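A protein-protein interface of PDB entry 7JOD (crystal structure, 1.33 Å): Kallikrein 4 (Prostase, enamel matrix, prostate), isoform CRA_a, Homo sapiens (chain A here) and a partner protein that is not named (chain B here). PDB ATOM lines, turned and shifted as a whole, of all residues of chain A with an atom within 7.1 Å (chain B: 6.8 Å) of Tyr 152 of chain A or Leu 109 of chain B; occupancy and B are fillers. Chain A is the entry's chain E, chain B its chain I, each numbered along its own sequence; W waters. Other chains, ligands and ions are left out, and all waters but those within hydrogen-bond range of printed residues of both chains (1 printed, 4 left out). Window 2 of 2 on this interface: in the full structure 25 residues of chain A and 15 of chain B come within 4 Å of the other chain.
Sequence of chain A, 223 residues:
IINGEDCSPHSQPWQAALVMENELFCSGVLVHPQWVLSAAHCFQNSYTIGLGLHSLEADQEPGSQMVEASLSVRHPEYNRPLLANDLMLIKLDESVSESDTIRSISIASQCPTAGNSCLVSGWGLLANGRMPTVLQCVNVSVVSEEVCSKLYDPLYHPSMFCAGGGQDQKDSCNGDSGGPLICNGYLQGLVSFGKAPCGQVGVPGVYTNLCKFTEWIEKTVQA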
ATOM      1  N   LEU A  83     -12.598  26.819  27.272  1.00  0.00           N
ATOM      2  CA  LEU A  83     -13.577  25.852  27.812  1.00  0.00           C
ATOM      3  C   LEU A  83     -13.192  24.388  27.566  1.00  0.00           C
ATOM      4  O   LEU A  83     -13.866  23.497  28.119  1.00  0.00           O
ATOM      5  CB  LEU A  83     -14.997  26.099  27.303  1.00  0.00           C
ATOM      6  CG  LEU A  83     -15.550  27.499  27.552  1.00  0.00           C
ATOM      7  CD1 LEU A  83     -16.940  27.648  26.955  1.00  0.00           C
ATOM      8  CD2 LEU A  83     -15.568  27.847  29.014  1.00  0.00           C
ATOM      9  N   VAL A 147     -24.435  18.563  15.021  1.00  0.00           N
ATOM     10  CA  VAL A 147     -25.387  19.497  15.675  1.00  0.00           C
ATOM     11  C   VAL A 147     -24.597  20.262  16.759  1.00  0.00           C
ATOM     12  O   VAL A 147     -24.790  21.472  16.899  1.00  0.00           O
ATOM     13  CB  VAL A 147     -26.587  18.729  16.240  1.00  0.00           C
ATOM     14  CG1 VAL A 147     -27.402  19.596  17.174  1.00  0.00           C
ATOM     15  CG2 VAL A 147     -27.443  18.147  15.122  1.00  0.00           C
ATOM     16  N   CYS A 148     -23.761  19.573  17.539  1.00  0.00           N
ATOM     17  CA  CYS A 148     -22.981  20.236  18.607  1.00  0.00           C
ATOM     18  C   CYS A 148     -22.130  21.382  18.009  1.00  0.00           C
ATOM     19  O   CYS A 148     -22.122  22.491  18.546  1.00  0.00           O
ATOM     20  CB  CYS A 148     -22.169  19.157  19.330  1.00  0.00           C
ATOM     21  SG  CYS A 148     -21.526  19.695  20.923  1.00  0.00           S
ATOM     22  N   SER A 149     -21.456  21.135  16.901  1.00  0.00           N
ATOM     23  CA  SER A 149     -20.569  22.142  16.276  1.00  0.00           C
ATOM     24  C   SER A 149     -21.401  23.287  15.707  1.00  0.00           C
ATOM     25  O   SER A 149     -21.037  24.469  15.871  1.00  0.00           O
ATOM     26  CB  SER A 149     -19.691  21.493  15.266  1.00  0.00           C
ATOM     27  OG  SER A 149     -20.431  21.027  14.147  1.00  0.00           O
ATOM     28  N   LYS A 150     -22.539  22.976  15.089  1.00  0.00           N
ATOM     29  CA  LYS A 150     -23.403  24.061  14.563  1.00  0.00           C
ATOM     30  C   LYS A 150     -23.835  25.001  15.682  1.00  0.00           C
ATOM     31  O   LYS A 150     -23.809  26.215  15.473  1.00  0.00           O
ATOM     32  CB  LYS A 150     -24.635  23.495  13.859  1.00  0.00           C
ATOM     33  CG  LYS A 150     -25.532  24.492  13.131  1.00  0.00           C
ATOM     34  CD  LYS A 150     -26.501  23.745  12.205  1.00  0.00           C
ATOM     35  CE  LYS A 150     -27.956  24.149  12.346  1.00  0.00           C
ATOM     36  NZ  LYS A 150     -28.358  25.147  11.328  1.00  0.00           N
ATOM     37  N   LEU A 151     -24.182  24.447  16.835  1.00  0.00           N
ATOM     38  CA  LEU A 151     -24.702  25.283  17.954  1.00  0.00           C
ATOM     39  C   LEU A 151     -23.541  26.026  18.630  1.00  0.00           C
ATOM     40  O   LEU A 151     -23.728  27.213  18.975  1.00  0.00           O
ATOM     41  CB  LEU A 151     -25.464  24.415  18.956  1.00  0.00           C
ATOM     42  CG  LEU A 151     -25.906  25.087  20.266  1.00  0.00           C
ATOM     43  CD1 LEU A 151     -26.822  26.266  20.008  1.00  0.00           C
ATOM     44  CD2 LEU A 151     -26.612  24.073  21.140  1.00  0.00           C
ATOM     45  N   TYR A 152     -22.411  25.361  18.832  1.00  0.00           N
ATOM     46  CA  TYR A 152     -21.351  25.889  19.724  1.00  0.00           C
ATOM     47  C   TYR A 152     -20.090  26.398  19.063  1.00  0.00           C
ATOM     48  O   TYR A 152     -19.362  27.113  19.752  1.00  0.00           O
ATOM     49  CB  TYR A 152     -21.039  24.890  20.832  1.00  0.00           C
ATOM     50  CG  TYR A 152     -22.118  24.795  21.894  1.00  0.00           C
ATOM     51  CD1 TYR A 152     -22.221  25.763  22.858  1.00  0.00           C
ATOM     52  CD2 TYR A 152     -22.991  23.733  21.962  1.00  0.00           C
ATOM     53  CE1 TYR A 152     -23.152  25.661  23.864  1.00  0.00           C
ATOM     54  CE2 TYR A 152     -23.961  23.622  22.943  1.00  0.00           C
ATOM     55  CZ  TYR A 152     -24.048  24.612  23.911  1.00  0.00           C
ATOM     56  OH  TYR A 152     -24.965  24.520  24.943  1.00  0.00           O
ATOM     57  N   ASP A 153     -19.861  26.155  17.769  1.00  0.00           N
ATOM     58  CA  ASP A 153     -18.698  26.818  17.111  1.00  0.00           C
ATOM     59  C   ASP A 153     -18.822  28.329  17.343  1.00  0.00           C
ATOM     60  O   ASP A 153     -19.916  28.892  17.250  1.00  0.00           O
ATOM     61  CB  ASP A 153     -18.671  26.501  15.618  1.00  0.00           C
ATOM     62  CG  ASP A 153     -18.139  25.146  15.186  1.00  0.00           C
ATOM     63  OD1 ASP A 153     -17.611  24.401  16.022  1.00  0.00           O
ATOM     64  OD2 ASP A 153     -18.228  24.862  13.965  1.00  0.00           O
ATOM     65  N   PRO A 154     -17.745  29.073  17.681  1.00  0.00           N
ATOM     66  CA  PRO A 154     -16.364  28.605  17.577  1.00  0.00           C
ATOM     67  C   PRO A 154     -15.733  27.963  18.820  1.00  0.00           C
ATOM     68  O   PRO A 154     -14.525  27.786  18.857  1.00  0.00           O
ATOM     69  CB  PRO A 154     -15.703  29.980  17.256  1.00  0.00           C
ATOM     70  CG  PRO A 154     -16.415  30.936  18.186  1.00  0.00           C
ATOM     71  CD  PRO A 154     -17.833  30.536  17.919  1.00  0.00           C
ATOM     72  N   LEU A 155     -16.571  27.588  19.774  1.00  0.00           N
ATOM     73  CA  LEU A 155     -16.118  27.018  21.052  1.00  0.00           C
ATOM     74  C   LEU A 155     -16.277  25.492  21.112  1.00  0.00           C
ATOM     75  O   LEU A 155     -15.879  24.898  22.117  1.00  0.00           O
ATOM     76  CB  LEU A 155     -16.807  27.729  22.231  1.00  0.00           C
ATOM     77  CG  LEU A 155     -16.411  29.182  22.427  1.00  0.00           C
ATOM     78  CD1 LEU A 155     -17.265  29.820  23.516  1.00  0.00           C
ATOM     79  CD2 LEU A 155     -14.921  29.263  22.735  1.00  0.00           C
ATOM     80  N   TYR A 156     -16.824  24.829  20.116  1.00  0.00           N
ATOM     81  CA  TYR A 156     -16.870  23.362  20.108  1.00  0.00           C
ATOM     82  C   TYR A 156     -15.466  22.820  19.837  1.00  0.00           C
ATOM     83  O   TYR A 156     -14.790  23.162  18.843  1.00  0.00           O
ATOM     84  CB  TYR A 156     -17.889  22.814  19.107  1.00  0.00           C
ATOM     85  CG  TYR A 156     -17.726  21.331  18.951  1.00  0.00           C
ATOM     86  CD1 TYR A 156     -18.084  20.433  19.939  1.00  0.00           C
ATOM     87  CD2 TYR A 156     -17.131  20.831  17.803  1.00  0.00           C
ATOM     88  CE1 TYR A 156     -17.814  19.080  19.808  1.00  0.00           C
ATOM     89  CE2 TYR A 156     -16.840  19.493  17.659  1.00  0.00           C
ATOM     90  CZ  TYR A 156     -17.175  18.609  18.662  1.00  0.00           C
ATOM     91  OH  TYR A 156     -16.866  17.263  18.546  1.00  0.00           O
ATOM     92  N   HIS A 157     -15.040  21.848  20.639  1.00  0.00           N
ATOM     93  CA  HIS A 157     -13.769  21.118  20.514  1.00  0.00           C
ATOM     94  C   HIS A 157     -14.050  19.650  20.783  1.00  0.00           C
ATOM     95  O   HIS A 157     -14.919  19.351  21.621  1.00  0.00           O
ATOM     96  CB  HIS A 157     -12.754  21.729  21.488  1.00  0.00           C
ATOM     97  CG  HIS A 157     -11.417  21.114  21.422  1.00  0.00           C
ATOM     98  ND1 HIS A 157     -10.998  20.135  22.310  1.00  0.00           N
ATOM     99  CD2 HIS A 157     -10.381  21.364  20.591  1.00  0.00           C
ATOM    100  CE1 HIS A 157      -9.774  19.776  22.017  1.00  0.00           C
ATOM    101  NE2 HIS A 157      -9.358  20.514  20.912  1.00  0.00           N
ATOM    102  N   MET A 160     -15.165  17.783  23.982  1.00  0.00           N
ATOM    103  CA  MET A 160     -16.538  18.061  24.406  1.00  0.00           C
ATOM    104  C   MET A 160     -17.500  17.144  23.666  1.00  0.00           C
ATOM    105  O   MET A 160     -17.199  16.793  22.516  1.00  0.00           O
ATOM    106  CB  MET A 160     -16.951  19.504  24.085  1.00  0.00           C
ATOM    107  CG  MET A 160     -16.010  20.551  24.665  1.00  0.00           C
ATOM    108  SD  MET A 160     -16.411  22.136  23.877  1.00  0.00           S
ATOM    109  CE  MET A 160     -15.160  23.157  24.656  1.00  0.00           C
ATOM    110  N   CYS A 162     -22.155  17.024  23.313  1.00  0.00           N
ATOM    111  CA  CYS A 162     -23.436  17.604  23.699  1.00  0.00           C
ATOM    112  C   CYS A 162     -24.443  16.505  24.004  1.00  0.00           C
ATOM    113  O   CYS A 162     -24.460  15.461  23.338  1.00  0.00           O
ATOM    114  CB  CYS A 162     -23.998  18.472  22.567  1.00  0.00           C
ATOM    115  SG  CYS A 162     -23.129  20.051  22.309  1.00  0.00           S
ATOM    116  N   PHE A 193     -20.450  22.757  30.761  1.00  0.00           N
ATOM    117  CA  PHE A 193     -21.011  24.095  30.532  1.00  0.00           C
ATOM    118  C   PHE A 193     -22.285  24.006  29.690  1.00  0.00           C
ATOM    119  O   PHE A 193     -22.597  22.957  29.140  1.00  0.00           O
ATOM    120  CB  PHE A 193     -19.964  25.078  29.950  1.00  0.00           C
ATOM    121  CG  PHE A 193     -19.568  24.829  28.507  1.00  0.00           C
ATOM    122  CD1 PHE A 193     -18.525  24.003  28.214  1.00  0.00           C
ATOM    123  CD2 PHE A 193     -20.213  25.498  27.474  1.00  0.00           C
ATOM    124  CE1 PHE A 193     -18.116  23.808  26.901  1.00  0.00           C
ATOM    125  CE2 PHE A 193     -19.825  25.274  26.173  1.00  0.00           C
ATOM    126  CZ  PHE A 193     -18.779  24.468  25.890  1.00  0.00           C
ATOM    127  N   GLY A 194     -22.953  25.126  29.552  1.00  0.00           N
ATOM    128  CA  GLY A 194     -24.106  25.201  28.650  1.00  0.00           C
ATOM    129  C   GLY A 194     -24.704  26.580  28.665  1.00  0.00           C
ATOM    130  O   GLY A 194     -24.017  27.545  29.075  1.00  0.00           O
ATOM    131  N   LYS A 195     -25.957  26.708  28.231  1.00  0.00           N
ATOM    132  CA  LYS A 195     -26.693  28.000  28.294  1.00  0.00           C
ATOM    133  C   LYS A 195     -27.609  28.093  29.550  1.00  0.00           C
ATOM    134  O   LYS A 195     -28.122  27.053  30.084  1.00  0.00           O
ATOM    135  CB  LYS A 195     -27.413  28.177  26.949  1.00  0.00           C
ATOM    136  CG  LYS A 195     -26.510  28.033  25.719  1.00  0.00           C
ATOM    137  CD  LYS A 195     -26.936  28.812  24.458  1.00  0.00           C
ATOM    138  CE  LYS A 195     -26.448  28.177  23.149  1.00  0.00           C
ATOM    139  NZ  LYS A 195     -26.331  29.111  22.003  1.00  0.00           N
ATOM    140  N   ALA A 196     -27.913  29.304  30.002  1.00  0.00           N
ATOM    141  CA  ALA A 196     -28.916  29.607  31.055  1.00  0.00           C
ATOM    142  C   ALA A 196     -29.954  30.534  30.431  1.00  0.00           C
ATOM    143  O   ALA A 196     -29.591  31.396  29.637  1.00  0.00           O
ATOM    144  CB  ALA A 196     -28.252  30.247  32.260  1.00  0.00           C
ATOM    145  N   VAL A 203     -31.427  23.169  22.858  1.00  0.00           N
ATOM    146  CA  VAL A 203     -30.125  23.638  23.416  1.00  0.00           C
ATOM    147  C   VAL A 203     -29.550  22.583  24.346  1.00  0.00           C
ATOM    148  O   VAL A 203     -29.750  22.606  25.554  1.00  0.00           O
ATOM    149  CB  VAL A 203     -30.249  24.987  24.135  1.00  0.00           C
ATOM    150  CG1 VAL A 203     -28.867  25.489  24.514  1.00  0.00           C
ATOM    151  CG2 VAL A 203     -30.996  26.021  23.295  1.00  0.00           C
ATOM    152  N   PRO A 204     -28.753  21.661  23.849  1.00  0.00           N
ATOM    153  CA  PRO A 204     -28.121  20.653  24.684  1.00  0.00           C
ATOM    154  C   PRO A 204     -27.012  21.285  25.524  1.00  0.00           C
ATOM    155  O   PRO A 204     -26.401  22.257  25.164  1.00  0.00           O
ATOM    156  CB  PRO A 204     -27.519  19.653  23.710  1.00  0.00           C
ATOM    157  CG  PRO A 204     -27.343  20.433  22.449  1.00  0.00           C
ATOM    158  CD  PRO A 204     -28.360  21.530  22.449  1.00  0.00           C
ATOM    159  N   GLY A 205     -26.793  20.642  26.656  1.00  0.00           N
ATOM    160  CA  GLY A 205     -25.630  20.943  27.481  1.00  0.00           C
ATOM    161  C   GLY A 205     -24.359  20.297  26.981  1.00  0.00           C
ATOM    162  O   GLY A 205     -24.405  19.358  26.156  1.00  0.00           O
ATOM    163  N   VAL A 206     -23.223  20.766  27.468  1.00  0.00           N
ATOM    164  CA  VAL A 206     -21.909  20.325  27.007  1.00  0.00           C
ATOM    165  C   VAL A 206     -21.199  19.588  28.144  1.00  0.00           C
ATOM    166  O   VAL A 206     -21.184  20.041  29.325  1.00  0.00           O
ATOM    167  CB  VAL A 206     -21.075  21.478  26.439  1.00  0.00           C
ATOM    168  CG1 VAL A 206     -19.804  20.925  25.843  1.00  0.00           C
ATOM    169  CG2 VAL A 206     -21.885  22.294  25.416  1.00  0.00           C
ATOM    170  N   GLU B  61     -22.178  36.363  34.919  1.00  0.00           N
ATOM    171  CA  GLU B  61     -22.588  35.087  34.286  1.00  0.00           C
ATOM    172  C   GLU B  61     -21.406  34.406  33.590  1.00  0.00           C
ATOM    173  O   GLU B  61     -20.719  35.031  32.775  1.00  0.00           O
ATOM    174  CB  GLU B  61     -23.687  35.320  33.247  1.00  0.00           C
ATOM    175  CG  GLU B  61     -25.045  35.830  33.723  1.00  0.00           C
ATOM    176  CD  GLU B  61     -26.086  35.963  32.609  1.00  0.00           C
ATOM    177  OE1 GLU B  61     -25.727  35.786  31.411  1.00  0.00           O
ATOM    178  OE2 GLU B  61     -27.266  36.182  32.938  1.00  0.00           O
ATOM    179  N   SER B  62     -21.276  33.130  33.854  1.00  0.00           N
ATOM    180  CA  SER B  62     -20.361  32.213  33.166  1.00  0.00           C
ATOM    181  C   SER B  62     -21.199  31.049  32.658  1.00  0.00           C
ATOM    182  O   SER B  62     -22.133  30.552  33.322  1.00  0.00           O
ATOM    183  CB  SER B  62     -19.334  31.657  34.131  1.00  0.00           C
ATOM    184  OG  SER B  62     -18.617  30.542  33.619  1.00  0.00           O
ATOM    185  N   PRO B  63     -20.860  30.485  31.468  1.00  0.00           N
ATOM    186  CA  PRO B  63     -21.560  29.285  31.012  1.00  0.00           C
ATOM    187  C   PRO B  63     -21.260  27.988  31.755  1.00  0.00           C
ATOM    188  O   PRO B  63     -21.992  27.011  31.641  1.00  0.00           O
ATOM    189  CB  PRO B  63     -21.103  29.207  29.547  1.00  0.00           C
ATOM    190  CG  PRO B  63     -19.704  29.760  29.549  1.00  0.00           C
ATOM    191  CD  PRO B  63     -19.793  30.936  30.544  1.00  0.00           C
ATOM    192  N   LEU B  64     -20.184  28.031  32.542  1.00  0.00           N
ATOM    193  CA  LEU B  64     -19.797  26.874  33.354  1.00  0.00           C
ATOM    194  C   LEU B  64     -20.955  26.519  34.299  1.00  0.00           C
ATOM    195  O   LEU B  64     -21.605  27.455  34.866  1.00  0.00           O
ATOM    196  CB  LEU B  64     -18.527  27.188  34.136  1.00  0.00           C
ATOM    197  CG  LEU B  64     -17.300  27.548  33.307  1.00  0.00           C
ATOM    198  CD1 LEU B  64     -16.200  28.088  34.209  1.00  0.00           C
ATOM    199  CD2 LEU B  64     -16.823  26.354  32.511  1.00  0.00           C
ATOM    200  N   ARG B  65     -21.171  25.233  34.515  1.00  0.00           N
ATOM    201  CA  ARG B  65     -22.326  24.785  35.339  1.00  0.00           C
ATOM    202  C   ARG B  65     -21.998  24.745  36.837  1.00  0.00           C
ATOM    203  O   ARG B  65     -22.428  23.809  37.553  1.00  0.00           O
ATOM    204  CB  ARG B  65     -22.926  23.524  34.714  1.00  0.00           C
ATOM    205  CG  ARG B  65     -24.058  23.995  33.820  1.00  0.00           C
ATOM    206  CD  ARG B  65     -24.458  23.187  32.685  1.00  0.00           C
ATOM    207  NE  ARG B  65     -25.590  23.899  32.128  1.00  0.00           N
ATOM    208  CZ  ARG B  65     -26.393  23.319  31.308  1.00  0.00           C
ATOM    209  NH1 ARG B  65     -26.128  22.063  30.963  1.00  0.00           N
ATOM    210  NH2 ARG B  65     -27.413  24.009  30.833  1.00  0.00           N
ATOM    211  N   PHE B  74     -13.953  34.004  32.464  1.00  0.00           N
ATOM    212  CA  PHE B  74     -14.563  35.029  31.579  1.00  0.00           C
ATOM    213  C   PHE B  74     -16.046  35.147  31.888  1.00  0.00           C
ATOM    214  O   PHE B  74     -16.775  34.112  31.955  1.00  0.00           O
ATOM    215  CB  PHE B  74     -14.349  34.645  30.122  1.00  0.00           C
ATOM    216  CG  PHE B  74     -13.012  35.042  29.577  1.00  0.00           C
ATOM    217  CD1 PHE B  74     -12.665  36.384  29.514  1.00  0.00           C
ATOM    218  CD2 PHE B  74     -12.127  34.093  29.115  1.00  0.00           C
ATOM    219  CE1 PHE B  74     -11.441  36.746  29.025  1.00  0.00           C
ATOM    220  CE2 PHE B  74     -10.910  34.475  28.575  1.00  0.00           C
ATOM    221  CZ  PHE B  74     -10.582  35.805  28.532  1.00  0.00           C
ATOM    222  N   ASN B  76     -19.847  37.485  31.432  1.00  0.00           N
ATOM    223  CA  ASN B  76     -20.769  38.575  31.063  1.00  0.00           C
ATOM    224  C   ASN B  76     -21.154  39.324  32.349  1.00  0.00           C
ATOM    225  O   ASN B  76     -21.313  38.662  33.401  1.00  0.00           O
ATOM    226  CB  ASN B  76     -21.999  38.059  30.316  1.00  0.00           C
ATOM    227  CG  ASN B  76     -21.719  37.757  28.855  1.00  0.00           C
ATOM    228  OD1 ASN B  76     -21.298  38.679  28.160  1.00  0.00           O
ATOM    229  ND2 ASN B  76     -21.931  36.512  28.465  1.00  0.00           N
ATOM    230  N   LYS B 107     -25.592  38.980  23.556  1.00  0.00           N
ATOM    231  CA  LYS B 107     -24.660  38.403  24.508  1.00  0.00           C
ATOM    232  C   LYS B 107     -23.950  37.225  23.858  1.00  0.00           C
ATOM    233  O   LYS B 107     -24.614  36.392  23.248  1.00  0.00           O
ATOM    234  CB  LYS B 107     -25.502  38.038  25.740  1.00  0.00           C
ATOM    235  CG  LYS B 107     -24.872  37.148  26.772  1.00  0.00           C
ATOM    236  CD  LYS B 107     -25.748  37.025  27.998  1.00  0.00           C
ATOM    237  CE  LYS B 107     -26.514  35.728  28.019  1.00  0.00           C
ATOM    238  NZ  LYS B 107     -27.343  35.613  29.240  1.00  0.00           N
ATOM    239  N   SER B 108     -22.646  37.160  23.994  1.00  0.00           N
ATOM    240  CA  SER B 108     -21.884  35.965  23.631  1.00  0.00           C
ATOM    241  C   SER B 108     -22.023  34.884  24.713  1.00  0.00           C
ATOM    242  O   SER B 108     -22.216  35.214  25.884  1.00  0.00           O
ATOM    243  CB  SER B 108     -20.429  36.323  23.293  1.00  0.00           C
ATOM    244  OG  SER B 108     -20.331  37.162  22.114  1.00  0.00           O
ATOM    245  N   LEU B 109     -21.816  33.636  24.386  1.00  0.00           N
ATOM    246  CA  LEU B 109     -21.792  32.529  25.364  1.00  0.00           C
ATOM    247  C   LEU B 109     -20.774  32.837  26.455  1.00  0.00           C
ATOM    248  O   LEU B 109     -20.996  32.528  27.626  1.00  0.00           O
ATOM    249  CB  LEU B 109     -21.429  31.209  24.686  1.00  0.00           C
ATOM    250  CG  LEU B 109     -21.441  29.983  25.590  1.00  0.00           C
ATOM    251  CD1 LEU B 109     -22.839  29.745  26.119  1.00  0.00           C
ATOM    252  CD2 LEU B 109     -20.957  28.776  24.822  1.00  0.00           C
ATOM    253  N   LEU B 110     -19.638  33.358  26.057  1.00  0.00           N
ATOM    254  CA  LEU B 110     -18.532  33.691  26.954  1.00  0.00           C
ATOM    255  C   LEU B 110     -18.242  35.176  26.824  1.00  0.00           C
ATOM    256  O   LEU B 110     -17.883  35.718  25.742  1.00  0.00           O
ATOM    257  CB  LEU B 110     -17.404  32.784  26.507  1.00  0.00           C
ATOM    258  CG  LEU B 110     -16.284  32.556  27.464  1.00  0.00           C
ATOM    259  CD1 LEU B 110     -16.763  31.883  28.716  1.00  0.00           C
ATOM    260  CD2 LEU B 110     -15.266  31.710  26.761  1.00  0.00           C
ATOM    261  N   GLY B 111     -18.427  35.887  27.930  1.00  0.00           N
ATOM    262  CA  GLY B 111     -18.226  37.336  27.931  1.00  0.00           C
ATOM    263  C   GLY B 111     -16.761  37.711  28.014  1.00  0.00           C
ATOM    264  O   GLY B 111     -15.877  36.857  28.140  1.00  0.00           O
ATOM    265  N   ARG B 130     -11.130  38.074  24.073  1.00  0.00           N
ATOM    266  CA  ARG B 130     -10.999  36.963  25.041  1.00  0.00           C
ATOM    267  C   ARG B 130      -9.596  36.360  24.957  1.00  0.00           C
ATOM    268  O   ARG B 130      -9.425  35.177  25.184  1.00  0.00           O
ATOM    269  CB  ARG B 130     -12.091  35.914  24.906  1.00  0.00           C
ATOM    270  CG  ARG B 130     -13.442  36.418  25.324  1.00  0.00           C
ATOM    271  CD  ARG B 130     -13.931  37.590  24.558  1.00  0.00           C
ATOM    272  NE  ARG B 130     -15.370  37.611  24.762  1.00  0.00           N
ATOM    273  CZ  ARG B 130     -16.182  38.453  24.179  1.00  0.00           C
ATOM    274  NH1 ARG B 130     -17.469  38.301  24.393  1.00  0.00           N
ATOM    275  NH2 ARG B 130     -15.699  39.391  23.361  1.00  0.00           N
HETATM  276  O   HOH W   1     -23.630  20.167  30.854  1.00  0.00           O
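Of the 13 printed residues of chain B, 4 touch a printed residue of chain A. Hydrophobic or aromatic side chains of chain B within 4 Å of the printed part of chain A: Pro 63 and Leu 109. Hydrophobic or aromatic side chains of chain A that line the printed part of chain B: Tyr 152 and Phe 193. Among the printed residues, 10 pairs touch across the chains.
Tyr 152 of chain A touches just one residue of chain B: Leu 109 (3.8 Å). Leu 109 of chain B touches three residues of chain A. Of the printed residues of chain B, Gly 194 of chain A touches Pro 63, Arg 65 and Leu 109. Printed residues of chain A within 4 Å of Arg 65 of chain B: Phe 193 (3.8 Å), Gly 194 (3.9 Å), Lys 195 (3.2 Å) and Gly 205 (3.7 Å). Of the printed residues of chain B, Lys 195 of chain A touches Arg 65 (3.2 Å). Printed residues of chain B within 4 Å of Gly 205 of chain A: Arg 65. Of the printed residues of chain A, Pro 63 of chain B touches Phe 193 and Gly 194. The nearest printed residue of chain B that does not touch Tyr 152 of chain A is Arg 65 of chain B (6.4 Å). The nearest printed residue of chain A that does not touch Leu 109 of chain B is Leu 155 of chain A (4.1 Å).
Tyr 152 of chain A touches Leu 109 of chain B (CD1 to CD2, 3.8 Å). O of Pro 63 of chain B touches CA of Phe 193 of chain A, at 3.3 Å. Phe 193 of chain A touches Leu 64 of chain B (CB to CA, 3.9 Å). Phe 193 of chain A touches Arg 65 of chain B (C to CD, 3.8 Å). Phe 193 of chain A touches Leu 109 of chain B. N of Gly 194 of chain A touches NE of Arg 65 of chain B, at 3.9 Å. CD1 of Leu 109 of chain B touches O of Gly 194 of chain A, at 3.9 Å. Gly 205 of chain A touches Arg 65 of chain B (CA to NH1, 3.7 Å).
Water W1 lies within hydrogen-bond range of the backbone carbonyl oxygen (O) of Val 206 of chain A (2.9 Å), the guanidinium group (NH1) of Arg 65 of chain B (3.1 Å) and the backbone carbonyl oxygen (O) of Phe 193 of chain A (3.4 Å).
N of Gly 194 of chain A sits at hydrogen-bond distance from O of Pro 63 of chain B (3.0 Å). The backbone carbonyl oxygen (O) of Lys 195 of chain A is in hydrogen-bond range of the guanidinium group (NH2) of Arg 65 of chain B, at 3.2 Å.
The side-chain hydroxyl of Tyr 152 of chain A lies within hydrogen-bond range of the backbone carbonyl oxygen of Pro 204 of chain A, at 2.7 Å. The backbone NH (N) of Val 206 of chain A sits at hydrogen-bond distance from the backbone carbonyl oxygen (O) of Phe 193 of chain A, 2.8 Å away. N of Leu 64 of chain B lies within hydrogen-bond range of OG of Ser 62 of chain B, at 3.1 Å. SG of Cys 148 of chain A forms a disulfide with SG of Cys 162 of chain A (2.1 Å).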
